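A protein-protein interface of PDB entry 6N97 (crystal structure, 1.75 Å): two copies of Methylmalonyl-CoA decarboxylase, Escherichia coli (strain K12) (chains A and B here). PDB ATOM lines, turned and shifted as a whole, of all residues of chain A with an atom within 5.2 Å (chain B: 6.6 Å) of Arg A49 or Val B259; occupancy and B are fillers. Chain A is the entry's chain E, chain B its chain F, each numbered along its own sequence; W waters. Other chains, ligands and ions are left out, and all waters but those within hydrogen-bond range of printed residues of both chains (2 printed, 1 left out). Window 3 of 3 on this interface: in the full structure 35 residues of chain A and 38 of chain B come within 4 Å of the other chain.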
ATOM      1  N   LYS A  13      -3.503 -19.460   0.040  1.00  0.00           N
ATOM      2  CA  LYS A  13      -2.889 -18.129   0.296  1.00  0.00           C
ATOM      3  C   LYS A  13      -3.193 -17.661   1.710  1.00  0.00           C
ATOM      4  O   LYS A  13      -2.650 -16.575   2.123  1.00  0.00           O
ATOM      5  CB  LYS A  13      -3.408 -17.155  -0.757  1.00  0.00           C
ATOM      6  CG  LYS A  13      -2.970 -17.483  -2.173  1.00  0.00           C
ATOM      7  CD  LYS A  13      -3.732 -16.744  -3.250  1.00  0.00           C
ATOM      8  CE  LYS A  13      -3.152 -16.985  -4.630  1.00  0.00           C
ATOM      9  NZ  LYS A  13      -4.164 -16.722  -5.690  1.00  0.00           N
ATOM     10  N   VAL A  14      -3.941 -18.447   2.485  1.00  0.00           N
ATOM     11  CA  VAL A  14      -4.285 -18.074   3.885  1.00  0.00           C
ATOM     12  C   VAL A  14      -3.431 -18.856   4.869  1.00  0.00           C
ATOM     13  O   VAL A  14      -3.328 -20.069   4.746  1.00  0.00           O
ATOM     14  CB  VAL A  14      -5.776 -18.295   4.149  1.00  0.00           C
ATOM     15  CG1 VAL A  14      -6.074 -18.055   5.618  1.00  0.00           C
ATOM     16  CG2 VAL A  14      -6.613 -17.406   3.252  1.00  0.00           C
ATOM     17  N   PRO A  46       5.513 -13.904  -0.864  1.00  0.00           N
ATOM     18  CA  PRO A  46       4.560 -13.503  -1.902  1.00  0.00           C
ATOM     19  C   PRO A  46       3.291 -14.343  -2.038  1.00  0.00           C
ATOM     20  O   PRO A  46       2.270 -13.802  -2.336  1.00  0.00           O
ATOM     21  CB  PRO A  46       5.347 -13.612  -3.233  1.00  0.00           C
ATOM     22  CG  PRO A  46       6.800 -13.521  -2.807  1.00  0.00           C
ATOM     23  CD  PRO A  46       6.890 -14.043  -1.379  1.00  0.00           C
ATOM     24  N   GLU A  47       3.408 -15.645  -1.827  1.00  0.00           N
ATOM     25  CA  GLU A  47       2.285 -16.588  -2.042  1.00  0.00           C
ATOM     26  C   GLU A  47       1.375 -16.649  -0.794  1.00  0.00           C
ATOM     27  O   GLU A  47       0.303 -17.290  -0.873  1.00  0.00           O
ATOM     28  CB  GLU A  47       2.841 -17.968  -2.406  1.00  0.00           C
ATOM     29  CG  GLU A  47       3.603 -18.663  -1.292  1.00  0.00           C
ATOM     30  CD  GLU A  47       5.081 -18.325  -1.114  1.00  0.00           C
ATOM     31  OE1 GLU A  47       5.738 -19.056  -0.300  1.00  0.00           O
ATOM     32  OE2 GLU A  47       5.580 -17.331  -1.733  1.00  0.00           O
ATOM     33  N   ILE A  48       1.754 -15.993   0.310  1.00  0.00           N
ATOM     34  CA  ILE A  48       0.835 -15.831   1.479  1.00  0.00           C
ATOM     35  C   ILE A  48       0.148 -14.465   1.357  1.00  0.00           C
ATOM     36  O   ILE A  48       0.884 -13.462   1.161  1.00  0.00           O
ATOM     37  CB  ILE A  48       1.583 -15.935   2.800  1.00  0.00           C
ATOM     38  CG1 ILE A  48       2.311 -17.299   2.890  1.00  0.00           C
ATOM     39  CG2 ILE A  48       0.619 -15.683   3.941  1.00  0.00           C
ATOM     40  CD1 ILE A  48       1.371 -18.464   2.851  1.00  0.00           C
ATOM     41  N   ARG A  49      -1.173 -14.420   1.501  1.00  0.00           N
ATOM     42  CA  ARG A  49      -1.931 -13.168   1.248  1.00  0.00           C
ATOM     43  C   ARG A  49      -2.723 -12.683   2.448  1.00  0.00           C
ATOM     44  O   ARG A  49      -3.145 -11.531   2.423  1.00  0.00           O
ATOM     45  CB  ARG A  49      -2.873 -13.388   0.069  1.00  0.00           C
ATOM     46  CG  ARG A  49      -2.137 -13.814  -1.177  1.00  0.00           C
ATOM     47  CD  ARG A  49      -1.115 -12.817  -1.693  1.00  0.00           C
ATOM     48  NE  ARG A  49      -0.649 -13.293  -2.978  1.00  0.00           N
ATOM     49  CZ  ARG A  49      -1.352 -13.210  -4.113  1.00  0.00           C
ATOM     50  NH1 ARG A  49      -2.498 -12.551  -4.154  1.00  0.00           N
ATOM     51  NH2 ARG A  49      -0.866 -13.747  -5.215  1.00  0.00           N
ATOM     52  N   CYS A  50      -2.982 -13.531   3.442  1.00  0.00           N
ATOM     53  CA  CYS A  50      -3.879 -13.181   4.565  1.00  0.00           C
ATOM     54  C   CYS A  50      -3.529 -14.075   5.750  1.00  0.00           C
ATOM     55  O   CYS A  50      -3.279 -15.274   5.527  1.00  0.00           O
ATOM     56  CB  CYS A  50      -5.345 -13.357   4.173  1.00  0.00           C
ATOM     57  SG  CYS A  50      -6.474 -12.542   5.333  1.00  0.00           S
ATOM     58  N   ILE A  51      -3.386 -13.501   6.937  1.00  0.00           N
ATOM     59  CA  ILE A  51      -3.090 -14.257   8.184  1.00  0.00           C
ATOM     60  C   ILE A  51      -4.334 -14.238   9.056  1.00  0.00           C
ATOM     61  O   ILE A  51      -4.980 -13.177   9.160  1.00  0.00           O
ATOM     62  CB  ILE A  51      -1.917 -13.605   8.950  1.00  0.00           C
ATOM     63  CG1 ILE A  51      -0.765 -13.236   8.017  1.00  0.00           C
ATOM     64  CG2 ILE A  51      -1.465 -14.457  10.129  1.00  0.00           C
ATOM     65  CD1 ILE A  51      -0.152 -14.421   7.349  1.00  0.00           C
ATOM     66  N   LYS A  97       0.392  -7.722   4.851  1.00  0.00           N
ATOM     67  CA  LYS A  97      -0.774  -8.570   4.529  1.00  0.00           C
ATOM     68  C   LYS A  97      -1.793  -8.308   5.631  1.00  0.00           C
ATOM     69  O   LYS A  97      -1.403  -8.023   6.768  1.00  0.00           O
ATOM     70  CB  LYS A  97      -0.365 -10.046   4.521  1.00  0.00           C
ATOM     71  CG  LYS A  97       0.816 -10.339   3.581  1.00  0.00           C
ATOM     72  CD  LYS A  97       1.323 -11.708   3.656  1.00  0.00           C
ATOM     73  CE  LYS A  97       2.731 -11.858   3.107  1.00  0.00           C
ATOM     74  NZ  LYS A  97       2.754 -11.550   1.645  1.00  0.00           N
ATOM     75  N   PRO A  98      -3.087  -8.444   5.339  1.00  0.00           N
ATOM     76  CA  PRO A  98      -4.108  -8.348   6.375  1.00  0.00           C
ATOM     77  C   PRO A  98      -3.899  -9.428   7.433  1.00  0.00           C
ATOM     78  O   PRO A  98      -3.599 -10.580   7.091  1.00  0.00           O
ATOM     79  CB  PRO A  98      -5.419  -8.527   5.617  1.00  0.00           C
ATOM     80  CG  PRO A  98      -5.068  -8.157   4.198  1.00  0.00           C
ATOM     81  CD  PRO A  98      -3.682  -8.699   4.013  1.00  0.00           C
ATOM     82  N   ILE A 198     -10.356 -12.232   0.403  1.00  0.00           N
ATOM     83  CA  ILE A 198      -9.337 -11.146   0.417  1.00  0.00           C
ATOM     84  C   ILE A 198      -8.129 -11.602  -0.392  1.00  0.00           C
ATOM     85  O   ILE A 198      -7.591 -10.796  -1.186  1.00  0.00           O
ATOM     86  CB  ILE A 198      -8.974 -10.777   1.866  1.00  0.00           C
ATOM     87  CG1 ILE A 198     -10.159 -10.143   2.601  1.00  0.00           C
ATOM     88  CG2 ILE A 198      -7.725  -9.930   1.901  1.00  0.00           C
ATOM     89  CD1 ILE A 198      -9.937  -9.924   4.093  1.00  0.00           C
ATOM     90  N   SER A 199      -7.750 -12.876  -0.268  1.00  0.00           N
ATOM     91  CA  SER A 199      -6.557 -13.446  -0.926  1.00  0.00           C
ATOM     92  C   SER A 199      -6.681 -13.452  -2.452  1.00  0.00           C
ATOM     93  O   SER A 199      -5.632 -13.637  -3.102  1.00  0.00           O
ATOM     94  CB  SER A 199      -6.220 -14.827  -0.356  1.00  0.00           C
ATOM     95  OG  SER A 199      -5.812 -14.703   1.013  1.00  0.00           O
ATOM     96  N   LYS A 201      -7.604 -10.767  -4.076  1.00  0.00           N
ATOM     97  CA  LYS A 201      -7.484  -9.335  -4.417  1.00  0.00           C
ATOM     98  C   LYS A 201      -5.993  -8.993  -4.579  1.00  0.00           C
ATOM     99  O   LYS A 201      -5.088  -9.798  -4.272  1.00  0.00           O
ATOM    100  CB  LYS A 201      -8.224  -8.504  -3.345  1.00  0.00           C
ATOM    101  CG  LYS A 201      -9.676  -8.886  -3.075  1.00  0.00           C
ATOM    102  CD  LYS A 201     -10.593  -8.834  -4.315  1.00  0.00           C
ATOM    103  CE  LYS A 201     -12.029  -9.200  -4.027  1.00  0.00           C
ATOM    104  NZ  LYS A 201     -12.896  -9.019  -5.215  1.00  0.00           N
ATOM    105  N   PRO A 203      -2.533  -7.893  -3.865  1.00  0.00           N
ATOM    106  CA  PRO A 203      -1.782  -7.797  -2.621  1.00  0.00           C
ATOM    107  C   PRO A 203      -0.941  -6.526  -2.482  1.00  0.00           C
ATOM    108  O   PRO A 203      -0.762  -6.053  -1.388  1.00  0.00           O
ATOM    109  CB  PRO A 203      -0.919  -9.070  -2.650  1.00  0.00           C
ATOM    110  CG  PRO A 203      -0.758  -9.369  -4.135  1.00  0.00           C
ATOM    111  CD  PRO A 203      -2.096  -9.005  -4.729  1.00  0.00           C
ATOM    112  N   GLU B 241       3.319  -5.468 -12.402  1.00  0.00           N
ATOM    113  CA  GLU B 241       2.553  -6.337 -13.340  1.00  0.00           C
ATOM    114  C   GLU B 241       1.108  -6.476 -12.861  1.00  0.00           C
ATOM    115  O   GLU B 241       0.202  -6.509 -13.708  1.00  0.00           O
ATOM    116  CB  GLU B 241       3.233  -7.690 -13.466  1.00  0.00           C
ATOM    117  CG  GLU B 241       4.628  -7.573 -14.063  1.00  0.00           C
ATOM    118  CD  GLU B 241       4.879  -8.367 -15.337  1.00  0.00           C
ATOM    119  OE1 GLU B 241       4.005  -9.195 -15.708  1.00  0.00           O
ATOM    120  OE2 GLU B 241       5.953  -8.145 -15.963  1.00  0.00           O
ATOM    121  N   ASP B 242       0.876  -6.578 -11.539  1.00  0.00           N
ATOM    122  CA  ASP B 242      -0.514  -6.723 -11.018  1.00  0.00           C
ATOM    123  C   ASP B 242      -1.365  -5.538 -11.455  1.00  0.00           C
ATOM    124  O   ASP B 242      -2.542  -5.738 -11.720  1.00  0.00           O
ATOM    125  CB  ASP B 242      -0.549  -6.895  -9.488  1.00  0.00           C
ATOM    126  CG  ASP B 242      -0.201  -8.281  -8.985  1.00  0.00           C
ATOM    127  OD1 ASP B 242      -0.066  -9.248  -9.842  1.00  0.00           O
ATOM    128  OD2 ASP B 242       0.005  -8.394  -7.761  1.00  0.00           O
ATOM    129  N   ASN B 257      -5.663 -12.395 -12.206  1.00  0.00           N
ATOM    130  CA  ASN B 257      -4.736 -13.316 -11.529  1.00  0.00           C
ATOM    131  C   ASN B 257      -3.581 -12.509 -10.937  1.00  0.00           C
ATOM    132  O   ASN B 257      -2.615 -12.255 -11.643  1.00  0.00           O
ATOM    133  CB  ASN B 257      -4.216 -14.418 -12.454  1.00  0.00           C
ATOM    134  CG  ASN B 257      -3.407 -15.424 -11.663  1.00  0.00           C
ATOM    135  OD1 ASN B 257      -3.840 -15.876 -10.602  1.00  0.00           O
ATOM    136  ND2 ASN B 257      -2.215 -15.747 -12.129  1.00  0.00           N
ATOM    137  N   PHE B 258      -3.701 -12.066  -9.691  1.00  0.00           N
ATOM    138  CA  PHE B 258      -2.649 -11.270  -9.019  1.00  0.00           C
ATOM    139  C   PHE B 258      -1.565 -12.202  -8.482  1.00  0.00           C
ATOM    140  O   PHE B 258      -1.913 -13.213  -7.914  1.00  0.00           O
ATOM    141  CB  PHE B 258      -3.269 -10.371  -7.952  1.00  0.00           C
ATOM    142  CG  PHE B 258      -4.280  -9.396  -8.488  1.00  0.00           C
ATOM    143  CD1 PHE B 258      -3.904  -8.466  -9.438  1.00  0.00           C
ATOM    144  CD2 PHE B 258      -5.575  -9.376  -8.005  1.00  0.00           C
ATOM    145  CE1 PHE B 258      -4.807  -7.531  -9.881  1.00  0.00           C
ATOM    146  CE2 PHE B 258      -6.483  -8.451  -8.477  1.00  0.00           C
ATOM    147  CZ  PHE B 258      -6.090  -7.528  -9.417  1.00  0.00           C
ATOM    148  N   VAL B 259      -0.297 -11.808  -8.584  1.00  0.00           N
ATOM    149  CA  VAL B 259       0.879 -12.647  -8.209  1.00  0.00           C
ATOM    150  C   VAL B 259       1.794 -11.921  -7.215  1.00  0.00           C
ATOM    151  O   VAL B 259       2.749 -12.544  -6.761  1.00  0.00           O
ATOM    152  CB  VAL B 259       1.629 -13.071  -9.493  1.00  0.00           C
ATOM    153  CG1 VAL B 259       0.744 -13.901 -10.408  1.00  0.00           C
ATOM    154  CG2 VAL B 259       2.208 -11.894 -10.264  1.00  0.00           C
ATOM    155  N   GLY B 260       1.552 -10.641  -6.880  1.00  0.00           N
ATOM    156  CA  GLY B 260       2.404  -9.924  -5.907  1.00  0.00           C
ATOM    157  C   GLY B 260       3.647  -9.283  -6.509  1.00  0.00           C
ATOM    158  O   GLY B 260       4.567  -8.945  -5.716  1.00  0.00           O
ATOM    159  N   HIS B 261       3.686  -9.033  -7.815  1.00  0.00           N
ATOM    160  CA  HIS B 261       4.723  -8.150  -8.418  1.00  0.00           C
ATOM    161  C   HIS B 261       4.109  -7.391  -9.579  1.00  0.00           C
ATOM    162  O   HIS B 261       4.860  -6.634 -10.257  1.00  0.00           O
ATOM    163  CB  HIS B 261       6.025  -8.921  -8.754  1.00  0.00           C
ATOM    164  CG  HIS B 261       5.881  -9.983  -9.791  1.00  0.00           C
ATOM    165  ND1 HIS B 261       5.933 -11.341  -9.480  1.00  0.00           N
ATOM    166  CD2 HIS B 261       5.697  -9.906 -11.129  1.00  0.00           C
ATOM    167  CE1 HIS B 261       5.807 -12.045 -10.596  1.00  0.00           C
ATOM    168  NE2 HIS B 261       5.635 -11.185 -11.620  1.00  0.00           N
ATOM    169  OXT HIS B 261       2.878  -7.525  -9.802  1.00  0.00           O
HETATM  170  O   HOH W   1      -4.487 -13.725  -5.692  1.00  0.00           O
HETATM  171  O   HOH W   2      -2.852 -15.671  -8.329  1.00  0.00           O
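The guanidinium group of Arg A49 lies within hydrogen-bond range of the backbone carbonyl oxygen of Phe B258 (2.9 Å).
O of Lys A13 sits at hydrogen-bond distance from N of Arg A49 (2.7 Å).
The backbone carbonyl oxygen (O) of Pro A46 is in hydrogen-bond range of the guanidinium group (NE) of Arg A49, 3.0 Å away.
NH1 of Arg A49 lies within hydrogen-bond range of O of Ser A199 (3.5 Å).
The backbone NH (N) of Val B259 sits at hydrogen-bond distance from the side-chain carboxylate (OD1) of Asp B242, at 2.9 Å.
N of Gly B260 lies within hydrogen-bond range of OD2 of Asp B242, 2.9 Å away.
The backbone NH (N) of Asp B242 lies within hydrogen-bond range of the chain-end carboxylate (OXT) of His B261, 2.8 Å away.
NH2 of Arg A49 touches CA of Val B259, at 3.6 Å.
Lys A201 touches Phe B258.
Asp B242 touches Pro A203 (OD2 to CD, 3.7 Å).
Pro A203 touches Phe B258 (CD to CB, 3.7 Å).
CA of Gly B260 touches CG of Pro A203, 3.7 Å away.
Arg A49 touches just these residues of chain B: Phe B258 and Val B259.
Printed residues of chain B within 4 Å of Lys A201: Phe B258.
Printed residues of chain A within 4 Å of Gly B260: Pro A203 (3.7 Å).
The nearest residue of chain B that does not touch Arg A49 is Gly B260 (4.3 Å).
The nearest residue of chain A that does not touch Val B259 is Pro A46 (4.5 Å).
Of the 14 printed residues of chain A, 3 touch a printed residue of chain B.
Of the 7 printed residues of chain B, 4 touch a printed residue of chain A.
Along chain B the printed residues that touch a printed residue of chain A span positions 242 to 260.
Among the printed residues, no Asp or Glu carboxylate lies within 4 Å of a Lys or Arg side-chain nitrogen of the other chain.
No position is printed for both chains.
Of the 6 pairs that touch across the chains among the printed residues, none has its exchanged pair printed and touching as well.
Water W2 lies within hydrogen-bond range of the side-chain amide oxygen of Asn B257 (2.5 Å), the backbone carbonyl oxygen of Phe B258 (2.7 Å) and the side-chain amino group of Lys A13 (3.1 Å).
Water W1 lies within hydrogen-bond range of NH1 of Arg A49 (2.8 Å), O of Ser A199 (2.8 Å), NZ of Lys A13 (3.0 Å) and O of Phe B258 (3.4 Å).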
